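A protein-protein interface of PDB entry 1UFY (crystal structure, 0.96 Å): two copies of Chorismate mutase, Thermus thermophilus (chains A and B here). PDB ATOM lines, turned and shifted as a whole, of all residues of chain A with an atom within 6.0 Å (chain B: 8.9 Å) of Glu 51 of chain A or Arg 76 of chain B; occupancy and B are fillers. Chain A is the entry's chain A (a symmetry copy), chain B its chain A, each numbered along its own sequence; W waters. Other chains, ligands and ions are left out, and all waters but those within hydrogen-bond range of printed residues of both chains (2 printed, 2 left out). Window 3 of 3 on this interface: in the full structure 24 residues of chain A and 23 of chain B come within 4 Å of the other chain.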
ATOM      1  N   VAL A  49      -8.431 -17.584 -33.780  1.00  0.00           N
ATOM      2  CA  VAL A  49      -9.329 -18.696 -33.877  1.00  0.00           C
ATOM      3  C   VAL A  49      -9.888 -18.982 -32.484  1.00  0.00           C
ATOM      4  O   VAL A  49      -9.179 -18.851 -31.472  1.00  0.00           O
ATOM      5  CB  VAL A  49      -8.818 -20.031 -34.510  1.00  0.00           C
ATOM      6  CG1 VAL A  49      -8.574 -19.802 -35.962  1.00  0.00           C
ATOM      7  CG2 VAL A  49      -7.649 -20.476 -33.731  1.00  0.00           C
ATOM      8  N   THR A  50     -11.134 -19.406 -32.422  1.00  0.00           N
ATOM      9  CA  THR A  50     -11.712 -19.857 -31.177  1.00  0.00           C
ATOM     10  C   THR A  50     -11.056 -21.155 -30.736  1.00  0.00           C
ATOM     11  O   THR A  50     -10.443 -21.883 -31.523  1.00  0.00           O
ATOM     12  CB  THR A  50     -13.223 -19.954 -31.327  1.00  0.00           C
ATOM     13  OG1 THR A  50     -13.557 -20.642 -32.524  1.00  0.00           O
ATOM     14  CG2 THR A  50     -13.847 -18.558 -31.440  1.00  0.00           C
ATOM     15  N   GLU A  51     -11.200 -21.481 -29.435  1.00  0.00           N
ATOM     16  CA  GLU A  51     -10.504 -22.621 -28.826  1.00  0.00           C
ATOM     17  C   GLU A  51     -10.973 -23.960 -29.344  1.00  0.00           C
ATOM     18  O   GLU A  51     -10.251 -24.962 -29.188  1.00  0.00           O
ATOM     19  CB  GLU A  51     -10.433 -22.464 -27.315  1.00  0.00           C
ATOM     20  CG  GLU A  51      -9.487 -21.243 -26.931  1.00  0.00           C
ATOM     21  CD  GLU A  51      -8.655 -21.490 -25.696  1.00  0.00           C
ATOM     22  OE1 GLU A  51      -9.115 -22.393 -24.990  1.00  0.00           O
ATOM     23  OE2 GLU A  51      -7.623 -20.836 -25.436  1.00  0.00           O
ATOM     24  N   ASP A  52     -12.101 -24.017 -30.015  1.00  0.00           N
ATOM     25  CA  ASP A  52     -12.657 -25.188 -30.647  1.00  0.00           C
ATOM     26  C   ASP A  52     -12.140 -25.464 -32.043  1.00  0.00           C
ATOM     27  O   ASP A  52     -12.581 -26.394 -32.692  1.00  0.00           O
ATOM     28  CB  ASP A  52     -14.167 -25.054 -30.601  1.00  0.00           C
ATOM     29  CG  ASP A  52     -14.692 -23.752 -31.159  1.00  0.00           C
ATOM     30  OD1 ASP A  52     -13.923 -23.120 -31.920  1.00  0.00           O
ATOM     31  OD2 ASP A  52     -15.844 -23.367 -30.926  1.00  0.00           O
ATOM     32  N   LEU A  53     -11.169 -24.637 -32.516  1.00  0.00           N
ATOM     33  CA  LEU A  53     -10.504 -24.840 -33.805  1.00  0.00           C
ATOM     34  C   LEU A  53      -8.992 -25.013 -33.555  1.00  0.00           C
ATOM     35  O   LEU A  53      -8.320 -24.009 -33.308  1.00  0.00           O
ATOM     36  CB  LEU A  53     -10.773 -23.709 -34.786  1.00  0.00           C
ATOM     37  CG  LEU A  53     -12.185 -23.495 -35.195  1.00  0.00           C
ATOM     38  CD1 LEU A  53     -12.339 -22.255 -36.098  1.00  0.00           C
ATOM     39  CD2 LEU A  53     -12.748 -24.697 -35.958  1.00  0.00           C
ATOM     40  N   THR A  54      -8.487 -26.179 -33.653  1.00  0.00           N
ATOM     41  CA  THR A  54      -7.048 -26.447 -33.519  1.00  0.00           C
ATOM     42  C   THR A  54      -6.453 -27.171 -34.692  1.00  0.00           C
ATOM     43  O   THR A  54      -5.253 -27.414 -34.643  1.00  0.00           O
ATOM     44  CB  THR A  54      -6.736 -27.219 -32.223  1.00  0.00           C
ATOM     45  OG1 THR A  54      -7.442 -28.417 -32.198  1.00  0.00           O
ATOM     46  CG2 THR A  54      -7.083 -26.372 -31.028  1.00  0.00           C
ATOM     47  N   ALA A  75      -3.365 -16.110 -33.241  1.00  0.00           N
ATOM     48  CA  ALA A  75      -3.536 -16.264 -31.837  1.00  0.00           C
ATOM     49  C   ALA A  75      -4.910 -16.872 -31.519  1.00  0.00           C
ATOM     50  O   ALA A  75      -5.733 -17.055 -32.405  1.00  0.00           O
ATOM     51  CB  ALA A  75      -3.316 -14.962 -31.123  1.00  0.00           C
ATOM     52  N   ARG A  76      -5.132 -17.198 -30.260  1.00  0.00           N
ATOM     53  CA  ARG A  76      -6.381 -17.774 -29.801  1.00  0.00           C
ATOM     54  C   ARG A  76      -7.305 -16.685 -29.217  1.00  0.00           C
ATOM     55  O   ARG A  76      -6.852 -15.863 -28.444  1.00  0.00           O
ATOM     56  CB  ARG A  76      -6.093 -18.856 -28.794  1.00  0.00           C
ATOM     57  CG  ARG A  76      -5.105 -19.882 -29.326  1.00  0.00           C
ATOM     58  CD  ARG A  76      -5.013 -21.103 -28.425  1.00  0.00           C
ATOM     59  NE  ARG A  76      -6.002 -22.076 -28.755  1.00  0.00           N
ATOM     60  CZ  ARG A  76      -6.194 -23.212 -28.057  1.00  0.00           C
ATOM     61  NH1 ARG A  76      -5.493 -23.462 -26.954  1.00  0.00           N
ATOM     62  NH2 ARG A  76      -7.084 -24.047 -28.442  1.00  0.00           N
ATOM     63  N   GLU A  77      -8.599 -16.762 -29.539  1.00  0.00           N
ATOM     64  CA  GLU A  77      -9.631 -15.869 -29.026  1.00  0.00           C
ATOM     65  C   GLU A  77     -10.101 -16.245 -27.629  1.00  0.00           C
ATOM     66  O   GLU A  77     -10.029 -17.401 -27.230  1.00  0.00           O
ATOM     67  CB  GLU A  77     -10.873 -15.919 -29.966  1.00  0.00           C
ATOM     68  CG  GLU A  77     -12.059 -15.085 -29.578  1.00  0.00           C
ATOM     69  CD  GLU A  77     -11.830 -13.591 -29.453  1.00  0.00           C
ATOM     70  OE1 GLU A  77     -11.327 -13.037 -28.442  1.00  0.00           O
ATOM     71  OE2 GLU A  77     -12.175 -12.817 -30.383  1.00  0.00           O
ATOM     72  N   VAL A  78     -10.649 -15.287 -26.884  1.00  0.00           N
ATOM     73  CA  VAL A  78     -11.215 -15.517 -25.537  1.00  0.00           C
ATOM     74  C   VAL A  78     -12.454 -16.442 -25.619  1.00  0.00           C
ATOM     75  O   VAL A  78     -13.362 -16.139 -26.404  1.00  0.00           O
ATOM     76  CB  VAL A  78     -11.666 -14.165 -24.930  1.00  0.00           C
ATOM     77  CG1 VAL A  78     -12.169 -14.358 -23.482  1.00  0.00           C
ATOM     78  CG2 VAL A  78     -10.531 -13.110 -24.966  1.00  0.00           C
ATOM     79  N   PRO A  79     -12.504 -17.506 -24.812  1.00  0.00           N
ATOM     80  CA  PRO A  79     -13.661 -18.469 -24.860  1.00  0.00           C
ATOM     81  C   PRO A  79     -14.854 -18.034 -24.018  1.00  0.00           C
ATOM     82  O   PRO A  79     -15.157 -18.670 -22.979  1.00  0.00           O
ATOM     83  CB  PRO A  79     -13.049 -19.769 -24.404  1.00  0.00           C
ATOM     84  CG  PRO A  79     -12.017 -19.264 -23.381  1.00  0.00           C
ATOM     85  CD  PRO A  79     -11.445 -18.010 -24.026  1.00  0.00           C
ATOM     86  N   ASP B  14     -14.087 -12.115 -12.263  1.00  0.00           N
ATOM     87  CA  ASP B  14     -14.368 -12.474 -13.665  1.00  0.00           C
ATOM     88  C   ASP B  14     -15.857 -12.364 -13.943  1.00  0.00           C
ATOM     89  O   ASP B  14     -16.567 -13.382 -14.013  1.00  0.00           O
ATOM     90  CB  ASP B  14     -13.860 -13.872 -13.996  1.00  0.00           C
ATOM     91  CG  ASP B  14     -14.039 -14.213 -15.499  1.00  0.00           C
ATOM     92  OD1 ASP B  14     -14.318 -13.307 -16.259  1.00  0.00           O
ATOM     93  OD2 ASP B  14     -13.872 -15.406 -15.819  1.00  0.00           O
ATOM     94  N   ILE B  46      -6.054  -3.745 -30.233  1.00  0.00           N
ATOM     95  CA  ILE B  46      -5.911  -5.143 -29.900  1.00  0.00           C
ATOM     96  C   ILE B  46      -5.927  -5.291 -28.380  1.00  0.00           C
ATOM     97  O   ILE B  46      -5.281  -4.524 -27.676  1.00  0.00           O
ATOM     98  CB  ILE B  46      -4.635  -5.741 -30.517  1.00  0.00           C
ATOM     99  CG1 ILE B  46      -4.611  -5.478 -32.041  1.00  0.00           C
ATOM    100  CG2 ILE B  46      -4.517  -7.224 -30.155  1.00  0.00           C
ATOM    101  CD1 ILE B  46      -3.259  -5.784 -32.678  1.00  0.00           C
ATOM    102  N   PHE B  47      -6.655  -6.254 -27.888  1.00  0.00           N
ATOM    103  CA  PHE B  47      -6.768  -6.544 -26.468  1.00  0.00           C
ATOM    104  C   PHE B  47      -6.196  -7.919 -26.156  1.00  0.00           C
ATOM    105  O   PHE B  47      -6.364  -8.855 -26.977  1.00  0.00           O
ATOM    106  CB  PHE B  47      -8.238  -6.572 -26.039  1.00  0.00           C
ATOM    107  CG  PHE B  47      -9.013  -5.321 -26.327  1.00  0.00           C
ATOM    108  CD1 PHE B  47      -9.659  -5.127 -27.511  1.00  0.00           C
ATOM    109  CD2 PHE B  47      -9.103  -4.308 -25.399  1.00  0.00           C
ATOM    110  CE1 PHE B  47     -10.360  -3.983 -27.784  1.00  0.00           C
ATOM    111  CE2 PHE B  47      -9.794  -3.148 -25.656  1.00  0.00           C
ATOM    112  CZ  PHE B  47     -10.435  -3.000 -26.849  1.00  0.00           C
ATOM    113  N   THR B  48      -5.679  -8.102 -24.954  1.00  0.00           N
ATOM    114  CA  THR B  48      -5.469  -9.410 -24.424  1.00  0.00           C
ATOM    115  C   THR B  48      -6.093  -9.484 -23.026  1.00  0.00           C
ATOM    116  O   THR B  48      -6.189  -8.490 -22.293  1.00  0.00           O
ATOM    117  CB  THR B  48      -4.047  -9.896 -24.380  1.00  0.00           C
ATOM    118  OG1 THR B  48      -3.341  -9.198 -23.377  1.00  0.00           O
ATOM    119  CG2 THR B  48      -3.362  -9.828 -25.689  1.00  0.00           C
ATOM    120  N   VAL B  49      -6.500 -10.701 -22.648  1.00  0.00           N
ATOM    121  CA  VAL B  49      -6.980 -10.983 -21.328  1.00  0.00           C
ATOM    122  C   VAL B  49      -6.213 -12.189 -20.788  1.00  0.00           C
ATOM    123  O   VAL B  49      -5.887 -13.126 -21.536  1.00  0.00           O
ATOM    124  CB  VAL B  49      -8.512 -11.207 -21.110  1.00  0.00           C
ATOM    125  CG1 VAL B  49      -9.217  -9.916 -21.342  1.00  0.00           C
ATOM    126  CG2 VAL B  49      -8.927 -12.325 -21.976  1.00  0.00           C
ATOM    127  N   THR B  50      -5.955 -12.197 -19.496  1.00  0.00           N
ATOM    128  CA  THR B  50      -5.379 -13.355 -18.852  1.00  0.00           C
ATOM    129  C   THR B  50      -6.379 -14.501 -18.845  1.00  0.00           C
ATOM    130  O   THR B  50      -7.590 -14.316 -18.993  1.00  0.00           O
ATOM    131  CB  THR B  50      -4.881 -12.967 -17.468  1.00  0.00           C
ATOM    132  OG1 THR B  50      -5.874 -12.224 -16.775  1.00  0.00           O
ATOM    133  CG2 THR B  50      -3.650 -12.058 -17.569  1.00  0.00           C
ATOM    134  N   GLU B  51      -5.867 -15.732 -18.645  1.00  0.00           N
ATOM    135  CA  GLU B  51      -6.680 -16.950 -18.758  1.00  0.00           C
ATOM    136  C   GLU B  51      -7.732 -17.075 -17.682  1.00  0.00           C
ATOM    137  O   GLU B  51      -8.693 -17.846 -17.855  1.00  0.00           O
ATOM    138  CB  GLU B  51      -5.795 -18.166 -18.988  1.00  0.00           C
ATOM    139  CG  GLU B  51      -5.105 -18.084 -20.419  1.00  0.00           C
ATOM    140  CD  GLU B  51      -4.991 -19.420 -21.112  1.00  0.00           C
ATOM    141  OE1 GLU B  51      -5.081 -20.368 -20.326  1.00  0.00           O
ATOM    142  OE2 GLU B  51      -4.817 -19.529 -22.344  1.00  0.00           O
ATOM    143  N   ASP B  52      -7.644 -16.304 -16.620  1.00  0.00           N
ATOM    144  CA  ASP B  52      -8.596 -16.232 -15.541  1.00  0.00           C
ATOM    145  C   ASP B  52      -9.759 -15.291 -15.779  1.00  0.00           C
ATOM    146  O   ASP B  52     -10.593 -15.109 -14.912  1.00  0.00           O
ATOM    147  CB  ASP B  52      -7.826 -15.898 -14.279  1.00  0.00           C
ATOM    148  CG  ASP B  52      -6.941 -14.678 -14.396  1.00  0.00           C
ATOM    149  OD1 ASP B  52      -7.211 -13.880 -15.323  1.00  0.00           O
ATOM    150  OD2 ASP B  52      -6.042 -14.451 -13.578  1.00  0.00           O
ATOM    151  N   LEU B  53      -9.821 -14.682 -16.993  1.00  0.00           N
ATOM    152  CA  LEU B  53     -10.936 -13.826 -17.403  1.00  0.00           C
ATOM    153  C   LEU B  53     -11.580 -14.430 -18.666  1.00  0.00           C
ATOM    154  O   LEU B  53     -11.003 -14.283 -19.746  1.00  0.00           O
ATOM    155  CB  LEU B  53     -10.511 -12.384 -17.638  1.00  0.00           C
ATOM    156  CG  LEU B  53      -9.964 -11.645 -16.472  1.00  0.00           C
ATOM    157  CD1 LEU B  53      -9.467 -10.240 -16.864  1.00  0.00           C
ATOM    158  CD2 LEU B  53     -11.005 -11.476 -15.363  1.00  0.00           C
ATOM    159  N   THR B  54     -12.702 -15.023 -18.555  1.00  0.00           N
ATOM    160  CA  THR B  54     -13.446 -15.562 -19.704  1.00  0.00           C
ATOM    161  C   THR B  54     -14.851 -15.046 -19.813  1.00  0.00           C
ATOM    162  O   THR B  54     -15.519 -15.451 -20.756  1.00  0.00           O
ATOM    163  CB  THR B  54     -13.460 -17.102 -19.694  1.00  0.00           C
ATOM    164  OG1 THR B  54     -14.021 -17.568 -18.510  1.00  0.00           O
ATOM    165  CG2 THR B  54     -12.059 -17.627 -19.863  1.00  0.00           C
ATOM    166  N   SER B  55     -15.312 -14.209 -18.917  1.00  0.00           N
ATOM    167  CA  SER B  55     -16.751 -13.924 -18.900  1.00  0.00           C
ATOM    168  C   SER B  55     -17.180 -12.928 -19.927  1.00  0.00           C
ATOM    169  O   SER B  55     -18.378 -12.810 -20.144  1.00  0.00           O
ATOM    170  CB  SER B  55     -17.197 -13.497 -17.510  1.00  0.00           C
ATOM    171  OG  SER B  55     -16.687 -12.214 -17.158  1.00  0.00           O
ATOM    172  N   PRO B  58     -13.536  -7.856 -24.223  1.00  0.00           N
ATOM    173  CA  PRO B  58     -13.224  -6.421 -24.122  1.00  0.00           C
ATOM    174  C   PRO B  58     -13.771  -5.627 -25.299  1.00  0.00           C
ATOM    175  O   PRO B  58     -14.121  -4.461 -25.112  1.00  0.00           O
ATOM    176  CB  PRO B  58     -11.704  -6.412 -24.039  1.00  0.00           C
ATOM    177  CG  PRO B  58     -11.331  -7.741 -23.597  1.00  0.00           C
ATOM    178  CD  PRO B  58     -12.333  -8.727 -24.052  1.00  0.00           C
ATOM    179  N   LEU B  73      -9.654  -6.426 -32.015  1.00  0.00           N
ATOM    180  CA  LEU B  73      -9.331  -7.851 -31.976  1.00  0.00           C
ATOM    181  C   LEU B  73      -8.891  -8.238 -30.557  1.00  0.00           C
ATOM    182  O   LEU B  73      -8.249  -7.417 -29.921  1.00  0.00           O
ATOM    183  CB  LEU B  73      -8.239  -8.170 -32.979  1.00  0.00           C
ATOM    184  CG  LEU B  73      -8.053  -9.632 -33.367  1.00  0.00           C
ATOM    185  CD1 LEU B  73      -9.179 -10.138 -34.245  1.00  0.00           C
ATOM    186  CD2 LEU B  73      -6.728  -9.806 -34.063  1.00  0.00           C
ATOM    187  N   SER B  74      -9.212  -9.419 -30.092  1.00  0.00           N
ATOM    188  CA  SER B  74      -8.818  -9.850 -28.780  1.00  0.00           C
ATOM    189  C   SER B  74      -8.185 -11.238 -28.789  1.00  0.00           C
ATOM    190  O   SER B  74      -8.463 -12.073 -29.660  1.00  0.00           O
ATOM    191  CB  SER B  74      -9.927  -9.818 -27.717  1.00  0.00           C
ATOM    192  OG  SER B  74     -11.042 -10.479 -28.091  1.00  0.00           O
ATOM    193  N   ALA B  75      -7.313 -11.465 -27.833  1.00  0.00           N
ATOM    194  CA  ALA B  75      -6.609 -12.695 -27.697  1.00  0.00           C
ATOM    195  C   ALA B  75      -6.297 -12.982 -26.222  1.00  0.00           C
ATOM    196  O   ALA B  75      -6.545 -12.155 -25.357  1.00  0.00           O
ATOM    197  CB  ALA B  75      -5.373 -12.703 -28.548  1.00  0.00           C
ATOM    198  N   ARG B  76      -5.774 -14.164 -25.951  1.00  0.00           N
ATOM    199  CA  ARG B  76      -5.418 -14.581 -24.609  1.00  0.00           C
ATOM    200  C   ARG B  76      -3.914 -14.352 -24.346  1.00  0.00           C
ATOM    201  O   ARG B  76      -3.098 -14.694 -25.180  1.00  0.00           O
ATOM    202  CB  ARG B  76      -5.800 -16.024 -24.415  1.00  0.00           C
ATOM    203  CG  ARG B  76      -7.258 -16.279 -24.768  1.00  0.00           C
ATOM    204  CD  ARG B  76      -7.715 -17.662 -24.330  1.00  0.00           C
ATOM    205  NE  ARG B  76      -8.177 -17.659 -22.980  1.00  0.00           N
ATOM    206  CZ  ARG B  76      -8.556 -18.769 -22.319  1.00  0.00           C
ATOM    207  NH1 ARG B  76      -8.459 -19.969 -22.886  1.00  0.00           N
ATOM    208  NH2 ARG B  76      -8.990 -18.673 -21.118  1.00  0.00           N
ATOM    209  N   GLU B  77      -3.585 -13.853 -23.151  1.00  0.00           N
ATOM    210  CA  GLU B  77      -2.216 -13.639 -22.696  1.00  0.00           C
ATOM    211  C   GLU B  77      -1.551 -14.910 -22.191  1.00  0.00           C
ATOM    212  O   GLU B  77      -2.218 -15.831 -21.735  1.00  0.00           O
ATOM    213  CB  GLU B  77      -2.216 -12.614 -21.521  1.00  0.00           C
ATOM    214  CG  GLU B  77      -0.891 -12.292 -20.896  1.00  0.00           C
ATOM    215  CD  GLU B  77       0.171 -11.709 -21.809  1.00  0.00           C
ATOM    216  OE1 GLU B  77       0.894 -12.395 -22.574  1.00  0.00           O
ATOM    217  OE2 GLU B  77       0.394 -10.471 -21.812  1.00  0.00           O
ATOM    218  N   VAL B  78      -0.220 -14.958 -22.208  1.00  0.00           N
ATOM    219  CA  VAL B  78       0.566 -16.097 -21.685  1.00  0.00           C
ATOM    220  C   VAL B  78       0.378 -16.230 -20.154  1.00  0.00           C
ATOM    221  O   VAL B  78       0.574 -15.231 -19.450  1.00  0.00           O
ATOM    222  CB  VAL B  78       2.071 -15.854 -21.963  1.00  0.00           C
ATOM    223  CG1 VAL B  78       2.911 -17.072 -21.520  1.00  0.00           C
ATOM    224  CG2 VAL B  78       2.336 -15.536 -23.456  1.00  0.00           C
ATOM    225  N   PRO B  79       0.046 -17.426 -19.659  1.00  0.00           N
ATOM    226  CA  PRO B  79      -0.187 -17.623 -18.183  1.00  0.00           C
ATOM    227  C   PRO B  79       1.089 -17.879 -17.391  1.00  0.00           C
ATOM    228  O   PRO B  79       1.303 -19.010 -16.890  1.00  0.00           O
ATOM    229  CB  PRO B  79      -1.160 -18.774 -18.138  1.00  0.00           C
ATOM    230  CG  PRO B  79      -0.693 -19.601 -19.347  1.00  0.00           C
ATOM    231  CD  PRO B  79      -0.362 -18.555 -20.402  1.00  0.00           C
ATOM    232  N   VAL B  87      -5.884  -9.447 -15.679  1.00  0.00           N
ATOM    233  CA  VAL B  87      -5.403  -8.260 -16.364  1.00  0.00           C
ATOM    234  C   VAL B  87      -6.012  -8.185 -17.756  1.00  0.00           C
ATOM    235  O   VAL B  87      -5.970  -9.146 -18.536  1.00  0.00           O
ATOM    236  CB  VAL B  87      -3.875  -8.233 -16.531  1.00  0.00           C
ATOM    237  CG1 VAL B  87      -3.419  -6.893 -17.059  1.00  0.00           C
ATOM    238  CG2 VAL B  87      -3.153  -8.534 -15.227  1.00  0.00           C
ATOM    239  N   ARG B  89      -5.220  -6.091 -21.063  1.00  0.00           N
ATOM    240  CA  ARG B  89      -4.177  -5.330 -21.736  1.00  0.00           C
ATOM    241  C   ARG B  89      -4.718  -4.787 -23.059  1.00  0.00           C
ATOM    242  O   ARG B  89      -5.497  -5.470 -23.743  1.00  0.00           O
ATOM    243  CB  ARG B  89      -2.928  -6.130 -21.971  1.00  0.00           C
ATOM    244  CG  ARG B  89      -2.216  -6.542 -20.700  1.00  0.00           C
ATOM    245  CD  ARG B  89      -1.059  -7.489 -20.954  1.00  0.00           C
ATOM    246  NE  ARG B  89      -0.182  -7.703 -19.815  1.00  0.00           N
ATOM    247  CZ  ARG B  89      -0.347  -8.620 -18.868  1.00  0.00           C
ATOM    248  NH1 ARG B  89      -1.392  -9.400 -18.807  1.00  0.00           N
ATOM    249  NH2 ARG B  89       0.591  -8.727 -17.913  1.00  0.00           N
HETATM  250  O   HOH W   1      -4.006 -15.991 -27.671  1.00  0.00           O
HETATM  251  O   HOH W   2      -5.498 -21.589 -23.951  1.00  0.00           O
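The side-chain carboxylate of Glu 77 of chain A lies within hydrogen-bond range of the side-chain hydroxyl of Ser 74 of chain B, 2.6 Å away. The guanidinium group (NH1) of Arg 76 of chain B lies within salt-bridge range of the side-chain carboxylate (OE2) of Glu 51 of chain A (2.8 Å). The backbone NH of Arg 76 of chain B is in hydrogen-bond range of the backbone carbonyl oxygen of Arg 76 of chain A, at 3.2 Å.
The backbone NH (N) of Thr 54 of chain B is in hydrogen-bond range of the side-chain carboxylate (OD2) of Asp 14 of chain B. N of Ala 75 of chain B is in hydrogen-bond range of O of Phe 47 of chain B (2.9 Å). The backbone NH (N) of Val 49 of chain B is in hydrogen-bond range of the backbone carbonyl oxygen (O) of Ala 75 of chain B, 3.1 Å away. OE2 of Glu 51 of chain B lies within salt-bridge range of NH1 of Arg 76 of chain B, at 3.7 Å. The backbone NH of Val 49 of chain A lies within hydrogen-bond range of the backbone carbonyl oxygen of Ala 75 of chain A, at 3.1 Å. The guanidinium group (NH1) of Arg 76 of chain A is in salt-bridge range of the side-chain carboxylate (OE2) of Glu 51 of chain A, at 3.7 Å.
CB of Ala 75 of chain A touches CB of Ala 75 of chain B, at 3.996 Å. Arg 76 of chain A touches Ala 75 of chain B (O to CA, 3.3 Å). Arg 76 of chain B touches Glu 77 of chain A (CD to O, 3.7 Å). Val 78 of chain A touches Val 49 of chain B (CG2 to CG2, 3.5 Å). Val 78 of chain A touches Leu 53 of chain B (CG1 to O, 3.9 Å). Pro 79 of chain A touches Thr 54 of chain B. Arg 76 of chain B touches Pro 79 of chain A (CZ to CD, 3.4 Å).
Glu 51 of chain A touches one residue of chain B. No residue of chain B comes within 4 Å of Thr 50 of chain A. Of the printed residues of chain A, Ser 74 of chain B touches Glu 77. Printed residues of chain A within 4 Å of Leu 53 of chain B: Val 78 (3.9 Å). Of the printed residues of chain A, Ala 75 of chain B touches Ala 75 (3.996 Å) and Arg 76 (3.3 Å). Of the printed residues of chain B, Arg 76 of chain A touches Ala 75 and Arg 76. Pro 79 of chain B touches none of the printed residues of chain A. Leu 53 of chain A touches none of the printed residues of chain B. The nearest residue of chain B that does not touch Glu 51 of chain A is Glu 51 of chain B (4.4 Å). The nearest residue of chain A that does not touch Arg 76 of chain B is Val 78 of chain A (4.1 Å).
Printed residues of chain A that touch a printed residue of chain B: Glu 51, Ala 75, Arg 76, Glu 77, Val 78 and Pro 79. Hydrophobic or aromatic side chains of chain A within 4 Å of the printed part of chain B: Ala 75, Val 78 and Pro 79. Printed residues of chain B that touch a printed residue of chain A: Val 49, Leu 53, Thr 54, Ser 74, Ala 75 and Arg 76. Along chain B the printed residues that touch a printed residue of chain A span positions 49 to 76. Among the printed residues, 10 pairs touch across the chains. Among the printed residues, Asp or Glu carboxylates within 4 Å of a Lys or Arg side-chain nitrogen of the other chain: Glu 51 of chain A with Arg 76 of chain B.
Glu 51 of chain A touches Arg 76 of chain B, but with the chains exchanged Arg 76 of chain A does not touch Glu 51 of chain B (6.1 Å). Arg 76 of chain B touches its own counterpart, Arg 76 of chain A. Val 78 of chain A touches Val 49 of chain B, but with the chains exchanged Val 49 of chain A does not touch Val 78 of chain B (13.5 Å). Val 78 of chain A touches Leu 53 of chain B, but with the chains exchanged Leu 53 of chain A does not touch Val 78 of chain B (16.5 Å). Positions printed for both chains: 49, 50, 51, 52, 53, 54, 75, 76, 77, 78 and 79.
Water W2 lies within hydrogen-bond range of the side-chain carboxylate of Glu 51 of chain A (2.7 Å) and the side-chain carboxylate of Glu 51 of chain B (2.7 Å). Water W1 bridges O of Arg 76 of chain A (3.0 Å) and O of Arg 76 of chain B (3.0 Å).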
